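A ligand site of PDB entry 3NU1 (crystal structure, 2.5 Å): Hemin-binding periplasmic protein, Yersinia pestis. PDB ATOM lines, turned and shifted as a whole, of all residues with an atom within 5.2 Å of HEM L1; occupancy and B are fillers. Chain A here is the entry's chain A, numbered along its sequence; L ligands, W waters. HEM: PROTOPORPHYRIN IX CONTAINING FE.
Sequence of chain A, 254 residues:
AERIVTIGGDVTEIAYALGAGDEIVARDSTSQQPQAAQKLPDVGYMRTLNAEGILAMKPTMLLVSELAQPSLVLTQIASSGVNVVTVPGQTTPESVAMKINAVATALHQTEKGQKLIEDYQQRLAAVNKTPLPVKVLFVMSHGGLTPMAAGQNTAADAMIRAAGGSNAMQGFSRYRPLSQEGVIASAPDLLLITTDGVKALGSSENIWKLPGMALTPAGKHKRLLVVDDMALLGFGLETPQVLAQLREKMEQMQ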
ATOM      1  N   SER A  29      28.504  -1.707 -31.478  1.00  0.00           N
ATOM      2  CA  SER A  29      29.441  -1.740 -30.355  1.00  0.00           C
ATOM      3  C   SER A  29      28.771  -1.407 -29.014  1.00  0.00           C
ATOM      4  O   SER A  29      29.147  -1.954 -27.985  1.00  0.00           O
ATOM      5  CB  SER A  29      30.600  -0.774 -30.568  1.00  0.00           C
ATOM      6  OG  SER A  29      31.411  -1.176 -31.652  1.00  0.00           O
ATOM      7  N   THR A  30      27.794  -0.505 -29.031  1.00  0.00           N
ATOM      8  CA  THR A  30      27.167  -0.082 -27.785  1.00  0.00           C
ATOM      9  C   THR A  30      26.177  -1.110 -27.265  1.00  0.00           C
ATOM     10  O   THR A  30      25.630  -0.970 -26.166  1.00  0.00           O
ATOM     11  CB  THR A  30      26.460   1.290 -27.916  1.00  0.00           C
ATOM     12  OG1 THR A  30      25.236   1.145 -28.658  1.00  0.00           O
ATOM     13  CG2 THR A  30      27.364   2.312 -28.606  1.00  0.00           C
ATOM     14  N   TYR A  45      30.449   1.048 -34.471  1.00  0.00           N
ATOM     15  CA  TYR A  45      29.963   1.918 -33.424  1.00  0.00           C
ATOM     16  C   TYR A  45      28.822   2.792 -33.934  1.00  0.00           C
ATOM     17  O   TYR A  45      28.939   3.412 -34.993  1.00  0.00           O
ATOM     18  CB  TYR A  45      31.117   2.768 -32.904  1.00  0.00           C
ATOM     19  CG  TYR A  45      30.748   3.858 -31.931  1.00  0.00           C
ATOM     20  CD1 TYR A  45      29.969   3.585 -30.811  1.00  0.00           C
ATOM     21  CD2 TYR A  45      31.206   5.152 -32.106  1.00  0.00           C
ATOM     22  CE1 TYR A  45      29.657   4.573 -29.898  1.00  0.00           C
ATOM     23  CE2 TYR A  45      30.887   6.161 -31.216  1.00  0.00           C
ATOM     24  CZ  TYR A  45      30.115   5.865 -30.115  1.00  0.00           C
ATOM     25  OH  TYR A  45      29.804   6.870 -29.228  1.00  0.00           O
ATOM     26  N   ARG A  47      27.816   5.676 -33.574  1.00  0.00           N
ATOM     27  CA  ARG A  47      28.054   7.065 -33.966  1.00  0.00           C
ATOM     28  C   ARG A  47      29.005   7.220 -35.163  1.00  0.00           C
ATOM     29  O   ARG A  47      29.188   8.306 -35.691  1.00  0.00           O
ATOM     30  CB  ARG A  47      28.534   7.906 -32.774  1.00  0.00           C
ATOM     31  CG  ARG A  47      27.450   8.156 -31.722  1.00  0.00           C
ATOM     32  CD  ARG A  47      27.960   8.993 -30.537  1.00  0.00           C
ATOM     33  NE  ARG A  47      26.892   9.280 -29.581  1.00  0.00           N
ATOM     34  CZ  ARG A  47      26.493   8.426 -28.641  1.00  0.00           C
ATOM     35  NH1 ARG A  47      27.071   7.238 -28.523  1.00  0.00           N
ATOM     36  NH2 ARG A  47      25.508   8.762 -27.807  1.00  0.00           N
ATOM     37  N   THR A  48      29.594   6.102 -35.593  1.00  0.00           N
ATOM     38  CA  THR A  48      30.442   6.112 -36.769  1.00  0.00           C
ATOM     39  C   THR A  48      30.161   4.886 -37.659  1.00  0.00           C
ATOM     40  O   THR A  48      31.092   4.188 -38.058  1.00  0.00           O
ATOM     41  CB  THR A  48      31.924   6.141 -36.378  1.00  0.00           C
ATOM     42  OG1 THR A  48      32.281   4.915 -35.739  1.00  0.00           O
ATOM     43  CG2 THR A  48      32.220   7.321 -35.431  1.00  0.00           C
ATOM     44  N   THR A  91      17.226  11.483 -24.292  1.00  0.00           N
ATOM     45  CA  THR A  91      17.799  11.050 -23.021  1.00  0.00           C
ATOM     46  C   THR A  91      16.906  11.537 -21.891  1.00  0.00           C
ATOM     47  O   THR A  91      17.200  12.520 -21.212  1.00  0.00           O
ATOM     48  CB  THR A  91      19.256  11.514 -22.823  1.00  0.00           C
ATOM     49  OG1 THR A  91      19.354  12.930 -22.978  1.00  0.00           O
ATOM     50  CG2 THR A  91      20.178  10.820 -23.841  1.00  0.00           C
ATOM     51  N   ALA A 150      31.027  15.529 -18.057  1.00  0.00           N
ATOM     52  CA  ALA A 150      29.791  15.801 -18.788  1.00  0.00           C
ATOM     53  C   ALA A 150      29.205  17.167 -18.474  1.00  0.00           C
ATOM     54  O   ALA A 150      28.976  17.508 -17.313  1.00  0.00           O
ATOM     55  CB  ALA A 150      28.763  14.725 -18.478  1.00  0.00           C
ATOM     56  N   THR A 154      23.694  15.885 -22.184  1.00  0.00           N
ATOM     57  CA  THR A 154      24.254  14.545 -22.183  1.00  0.00           C
ATOM     58  C   THR A 154      23.289  13.636 -21.420  1.00  0.00           C
ATOM     59  O   THR A 154      22.493  14.104 -20.612  1.00  0.00           O
ATOM     60  CB  THR A 154      25.640  14.507 -21.516  1.00  0.00           C
ATOM     61  OG1 THR A 154      25.541  15.003 -20.177  1.00  0.00           O
ATOM     62  CG2 THR A 154      26.628  15.360 -22.299  1.00  0.00           C
ATOM     63  N   ALA A 155      23.361  12.341 -21.712  1.00  0.00           N
ATOM     64  CA  ALA A 155      22.620  11.349 -20.949  1.00  0.00           C
ATOM     65  C   ALA A 155      23.000  11.417 -19.473  1.00  0.00           C
ATOM     66  O   ALA A 155      22.148  11.314 -18.598  1.00  0.00           O
ATOM     67  CB  ALA A 155      22.895   9.957 -21.496  1.00  0.00           C
ATOM     68  N   ALA A 156      24.292  11.597 -19.213  1.00  0.00           N
ATOM     69  CA  ALA A 156      24.777  11.673 -17.831  1.00  0.00           C
ATOM     70  C   ALA A 156      24.087  12.798 -17.071  1.00  0.00           C
ATOM     71  O   ALA A 156      23.582  12.595 -15.975  1.00  0.00           O
ATOM     72  CB  ALA A 156      26.289  11.857 -17.787  1.00  0.00           C
ATOM     73  N   ARG A 174      27.847  18.719 -23.863  1.00  0.00           N
ATOM     74  CA  ARG A 174      28.683  17.578 -24.195  1.00  0.00           C
ATOM     75  C   ARG A 174      29.824  17.463 -23.184  1.00  0.00           C
ATOM     76  O   ARG A 174      29.658  17.840 -22.030  1.00  0.00           O
ATOM     77  CB  ARG A 174      29.239  17.695 -25.617  1.00  0.00           C
ATOM     78  CG  ARG A 174      28.310  17.186 -26.705  1.00  0.00           C
ATOM     79  CD  ARG A 174      27.362  18.253 -27.212  1.00  0.00           C
ATOM     80  NE  ARG A 174      26.768  17.837 -28.482  1.00  0.00           N
ATOM     81  CZ  ARG A 174      25.697  17.056 -28.582  1.00  0.00           C
ATOM     82  NH1 ARG A 174      25.087  16.610 -27.493  1.00  0.00           N
ATOM     83  NH2 ARG A 174      25.231  16.740 -29.786  1.00  0.00           N
ATOM     84  N   TYR A 175      30.965  16.972 -23.632  1.00  0.00           N
ATOM     85  CA  TYR A 175      32.060  16.649 -22.730  1.00  0.00           C
ATOM     86  C   TYR A 175      33.252  17.583 -22.936  1.00  0.00           C
ATOM     87  O   TYR A 175      33.435  18.125 -24.027  1.00  0.00           O
ATOM     88  CB  TYR A 175      32.486  15.192 -22.905  1.00  0.00           C
ATOM     89  CG  TYR A 175      31.505  14.192 -22.325  1.00  0.00           C
ATOM     90  CD1 TYR A 175      30.307  13.925 -22.959  1.00  0.00           C
ATOM     91  CD2 TYR A 175      31.799  13.520 -21.154  1.00  0.00           C
ATOM     92  CE1 TYR A 175      29.407  13.018 -22.424  1.00  0.00           C
ATOM     93  CE2 TYR A 175      30.918  12.602 -20.614  1.00  0.00           C
ATOM     94  CZ  TYR A 175      29.721  12.356 -21.243  1.00  0.00           C
ATOM     95  OH  TYR A 175      28.836  11.450 -20.699  1.00  0.00           O
ATOM     96  N   ASP A 229      28.507   1.362 -17.689  1.00  0.00           N
ATOM     97  CA  ASP A 229      28.541   2.390 -18.720  1.00  0.00           C
ATOM     98  C   ASP A 229      27.216   2.586 -19.463  1.00  0.00           C
ATOM     99  O   ASP A 229      26.678   3.698 -19.503  1.00  0.00           O
ATOM    100  CB  ASP A 229      29.670   2.097 -19.696  1.00  0.00           C
ATOM    101  CG  ASP A 229      31.024   1.998 -18.991  1.00  0.00           C
ATOM    102  OD1 ASP A 229      31.182   1.099 -18.134  1.00  0.00           O
ATOM    103  OD2 ASP A 229      31.904   2.826 -19.284  1.00  0.00           O
ATOM    104  N   MET A 230      26.681   1.509 -20.045  1.00  0.00           N
ATOM    105  CA  MET A 230      25.471   1.630 -20.856  1.00  0.00           C
ATOM    106  C   MET A 230      24.218   1.657 -19.996  1.00  0.00           C
ATOM    107  O   MET A 230      23.201   2.199 -20.401  1.00  0.00           O
ATOM    108  CB  MET A 230      25.376   0.507 -21.895  1.00  0.00           C
ATOM    109  CG  MET A 230      26.430   0.602 -22.987  1.00  0.00           C
ATOM    110  SD  MET A 230      26.363   2.189 -23.838  1.00  0.00           S
ATOM    111  CE  MET A 230      24.667   2.193 -24.392  1.00  0.00           C
ATOM    112  N   LEU A 233      24.059   5.378 -19.155  1.00  0.00           N
ATOM    113  CA  LEU A 233      23.987   6.359 -20.230  1.00  0.00           C
ATOM    114  C   LEU A 233      23.050   5.971 -21.364  1.00  0.00           C
ATOM    115  O   LEU A 233      22.736   6.799 -22.233  1.00  0.00           O
ATOM    116  CB  LEU A 233      25.394   6.599 -20.786  1.00  0.00           C
ATOM    117  CG  LEU A 233      26.424   7.060 -19.746  1.00  0.00           C
ATOM    118  CD1 LEU A 233      27.855   6.781 -20.209  1.00  0.00           C
ATOM    119  CD2 LEU A 233      26.221   8.539 -19.351  1.00  0.00           C
ATOM    120  N   GLY A 234      22.601   4.723 -21.367  1.00  0.00           N
ATOM    121  CA  GLY A 234      21.881   4.174 -22.503  1.00  0.00           C
ATOM    122  C   GLY A 234      20.405   4.520 -22.530  1.00  0.00           C
ATOM    123  O   GLY A 234      19.754   4.400 -23.557  1.00  0.00           O
HETATM  124  CHA HEM L   1      29.293   9.754 -26.238  1.00  0.00           C
HETATM  125  CHB HEM L   1      33.188   9.480 -29.142  1.00  0.00           C
HETATM  126  CHC HEM L   1      33.134   4.660 -28.751  1.00  0.00           C
HETATM  127  CHD HEM L   1      29.379   4.878 -25.702  1.00  0.00           C
HETATM  128  C1A HEM L   1      30.365  10.099 -27.026  1.00  0.00           C
HETATM  129  C2A HEM L   1      30.794  11.450 -27.327  1.00  0.00           C
HETATM  130  C3A HEM L   1      31.874  11.369 -28.128  1.00  0.00           C
HETATM  131  C4A HEM L   1      32.154   9.974 -28.360  1.00  0.00           C
HETATM  132  CMA HEM L   1      32.701  12.542 -28.710  1.00  0.00           C
HETATM  133  CAA HEM L   1      30.098  12.720 -26.775  1.00  0.00           C
HETATM  134  CBA HEM L   1      30.131  13.881 -27.766  1.00  0.00           C
HETATM  135  CGA HEM L   1      28.979  13.716 -28.712  1.00  0.00           C
HETATM  136  O1A HEM L   1      27.995  13.052 -28.304  1.00  0.00           O
HETATM  137  O2A HEM L   1      29.058  14.257 -29.843  1.00  0.00           O
HETATM  138  C1B HEM L   1      33.470   8.153 -29.366  1.00  0.00           C
HETATM  139  C2B HEM L   1      34.391   7.592 -30.343  1.00  0.00           C
HETATM  140  C3B HEM L   1      34.365   6.255 -30.204  1.00  0.00           C
HETATM  141  C4B HEM L   1      33.426   5.939 -29.161  1.00  0.00           C
HETATM  142  CMB HEM L   1      35.259   8.399 -31.345  1.00  0.00           C
HETATM  143  CAB HEM L   1      35.141   5.183 -31.002  1.00  0.00           C
HETATM  144  CBB HEM L   1      35.822   5.465 -32.117  1.00  0.00           C
HETATM  145  C1C HEM L   1      32.120   4.303 -27.901  1.00  0.00           C
HETATM  146  C2C HEM L   1      31.753   2.943 -27.568  1.00  0.00           C
HETATM  147  C3C HEM L   1      30.737   2.989 -26.723  1.00  0.00           C
HETATM  148  C4C HEM L   1      30.388   4.391 -26.501  1.00  0.00           C
HETATM  149  CMC HEM L   1      32.441   1.658 -28.082  1.00  0.00           C
HETATM  150  CAC HEM L   1      30.067   1.737 -26.141  1.00  0.00           C
HETATM  151  CBC HEM L   1      29.300   1.819 -25.054  1.00  0.00           C
HETATM  152  C1D HEM L   1      28.963   6.194 -25.603  1.00  0.00           C
HETATM  153  C2D HEM L   1      27.773   6.632 -24.902  1.00  0.00           C
HETATM  154  C3D HEM L   1      27.742   8.160 -25.060  1.00  0.00           C
HETATM  155  C4D HEM L   1      28.909   8.485 -25.845  1.00  0.00           C
HETATM  156  CMD HEM L   1      26.772   5.747 -24.148  1.00  0.00           C
HETATM  157  CAD HEM L   1      26.667   9.116 -24.492  1.00  0.00           C
HETATM  158  CBD HEM L   1      27.223   9.900 -23.296  1.00  0.00           C
HETATM  159  CGD HEM L   1      26.193  10.855 -22.733  1.00  0.00           C
HETATM  160  O1D HEM L   1      25.175  11.166 -23.417  1.00  0.00           O
HETATM  161  O2D HEM L   1      26.380  11.334 -21.583  1.00  0.00           O
HETATM  162  NA  HEM L   1      31.213   9.226 -27.688  1.00  0.00           N
HETATM  163  NB  HEM L   1      32.892   7.103 -28.662  1.00  0.00           N
HETATM  164  NC  HEM L   1      31.263   5.159 -27.242  1.00  0.00           N
HETATM  165  ND  HEM L   1      29.585   7.314 -26.155  1.00  0.00           N
HETATM  166 FE   HEM L   1      31.073   7.213 -27.654  1.00  0.00          FE
HETATM  167  CHA HEM L   2      36.849   4.873 -27.776  1.00  0.00           C
HETATM  168  CHB HEM L   2      33.105   4.608 -24.705  1.00  0.00           C
HETATM  169  CHC HEM L   2      32.908   9.461 -24.602  1.00  0.00           C
HETATM  170  CHD HEM L   2      36.654   9.760 -27.726  1.00  0.00           C
HETATM  171  C1A HEM L   2      35.883   4.401 -26.913  1.00  0.00           C
HETATM  172  C2A HEM L   2      35.688   3.013 -26.579  1.00  0.00           C
HETATM  173  C3A HEM L   2      34.652   2.927 -25.728  1.00  0.00           C
HETATM  174  C4A HEM L   2      34.166   4.267 -25.507  1.00  0.00           C
HETATM  175  CMA HEM L   2      34.092   1.634 -25.089  1.00  0.00           C
HETATM  176  CAA HEM L   2      36.549   1.839 -27.092  1.00  0.00           C
HETATM  177  CBA HEM L   2      37.851   1.926 -26.293  1.00  0.00           C
HETATM  178  CGA HEM L   2      39.010   1.495 -27.156  1.00  0.00           C
HETATM  179  O1A HEM L   2      40.185   1.693 -26.728  1.00  0.00           O
HETATM  180  O2A HEM L   2      38.762   0.975 -28.280  1.00  0.00           O
HETATM  181  C1B HEM L   2      32.757   5.894 -24.391  1.00  0.00           C
HETATM  182  C2B HEM L   2      31.774   6.266 -23.410  1.00  0.00           C
HETATM  183  C3B HEM L   2      31.711   7.602 -23.369  1.00  0.00           C
HETATM  184  C4B HEM L   2      32.655   8.134 -24.338  1.00  0.00           C
HETATM  185  CMB HEM L   2      30.947   5.279 -22.551  1.00  0.00           C
HETATM  186  CAB HEM L   2      30.795   8.417 -22.432  1.00  0.00           C
HETATM  187  CBB HEM L   2      30.947   9.732 -22.330  1.00  0.00           C
HETATM  188  C1C HEM L   2      33.904   9.957 -25.441  1.00  0.00           C
HETATM  189  C2C HEM L   2      34.166  11.352 -25.718  1.00  0.00           C
HETATM  190  C3C HEM L   2      35.202  11.438 -26.568  1.00  0.00           C
HETATM  191  C4C HEM L   2      35.627  10.095 -26.877  1.00  0.00           C
HETATM  192  CMC HEM L   2      33.391  12.548 -25.104  1.00  0.00           C
HETATM  193  CAC HEM L   2      35.811  12.752 -27.113  1.00  0.00           C
HETATM  194  CBC HEM L   2      36.956  12.763 -27.810  1.00  0.00           C
HETATM  195  C1D HEM L   2      37.026   8.486 -28.102  1.00  0.00           C
HETATM  196  C2D HEM L   2      37.996   8.154 -29.123  1.00  0.00           C
HETATM  197  C3D HEM L   2      38.059   6.621 -29.127  1.00  0.00           C
HETATM  198  C4D HEM L   2      37.110   6.190 -28.118  1.00  0.00           C
HETATM  199  CMD HEM L   2      38.814   9.117 -30.009  1.00  0.00           C
HETATM  200  CAD HEM L   2      38.931   5.734 -30.049  1.00  0.00           C
HETATM  201  CBD HEM L   2      40.234   5.331 -29.377  1.00  0.00           C
HETATM  202  CGD HEM L   2      40.993   4.447 -30.336  1.00  0.00           C
HETATM  203  O1D HEM L   2      40.491   4.233 -31.483  1.00  0.00           O
HETATM  204  O2D HEM L   2      42.096   3.958 -29.969  1.00  0.00           O
HETATM  205  NA  HEM L   2      34.935   5.143 -26.245  1.00  0.00           N
HETATM  206  NB  HEM L   2      33.280   7.047 -24.942  1.00  0.00           N
HETATM  207  NC  HEM L   2      34.821   9.214 -26.178  1.00  0.00           N
HETATM  208  ND  HEM L   2      36.537   7.320 -27.529  1.00  0.00           N
HETATM  209 FE   HEM L   2      34.992   7.179 -26.116  1.00  0.00          FE
HETATM  210  O   HOH W   1      23.585  10.159 -25.244  1.00  0.00           O
HETATM  211  O   HOH W   2      26.608  12.766 -25.566  1.00  0.00           O
HETATM  212  O   HOH W   3      24.593   6.055 -26.569  1.00  0.00           O
HETATM  213  O   HOH W   4      31.851  16.171 -26.317  1.00  0.00           O
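OH of Tyr 45 lies close to NH1 of Arg 47 (2.8 Å).
Water W1 lies within hydrogen-bond range of an oxygen (O1D) of HEM L1 (2.6 Å) and the guanidinium group of Arg 47 (3.5 Å).
The guanidinium group (NH1) of Arg 47 lies close to a nitrogen (ND) of HEM L1, 3.5 Å away.
Residues that only touch HEM L1: Met 230, Thr 154, Leu 233, Thr 30, Arg 174 and Ser 29.
Hydrophobic or aromatic side chains within 4 Å of HEM L1: Tyr 45, Ala 155, Ala 156, Tyr 175, Met 230 and Leu 233.
11 residues have an atom within 4 Å of HEM L1: Ser 29, Thr 30, Tyr 45, Arg 47, Thr 154, Ala 155, Ala 156, Arg 174, Tyr 175, Met 230 and Leu 233.
OH of Tyr 45 binds FE of HEM L1 (2.1 Å).
O2D of HEM L1 is in hydrogen-bond range of N of Ala 156 (3.2 Å).
An oxygen (O2D) of HEM L1 lies within hydrogen-bond range of the side-chain hydroxyl (OH) of Tyr 175 (2.6 Å).
The backbone NH of Ala 155 is in hydrogen-bond range of an oxygen (O1D) of HEM L1 (2.8 Å).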
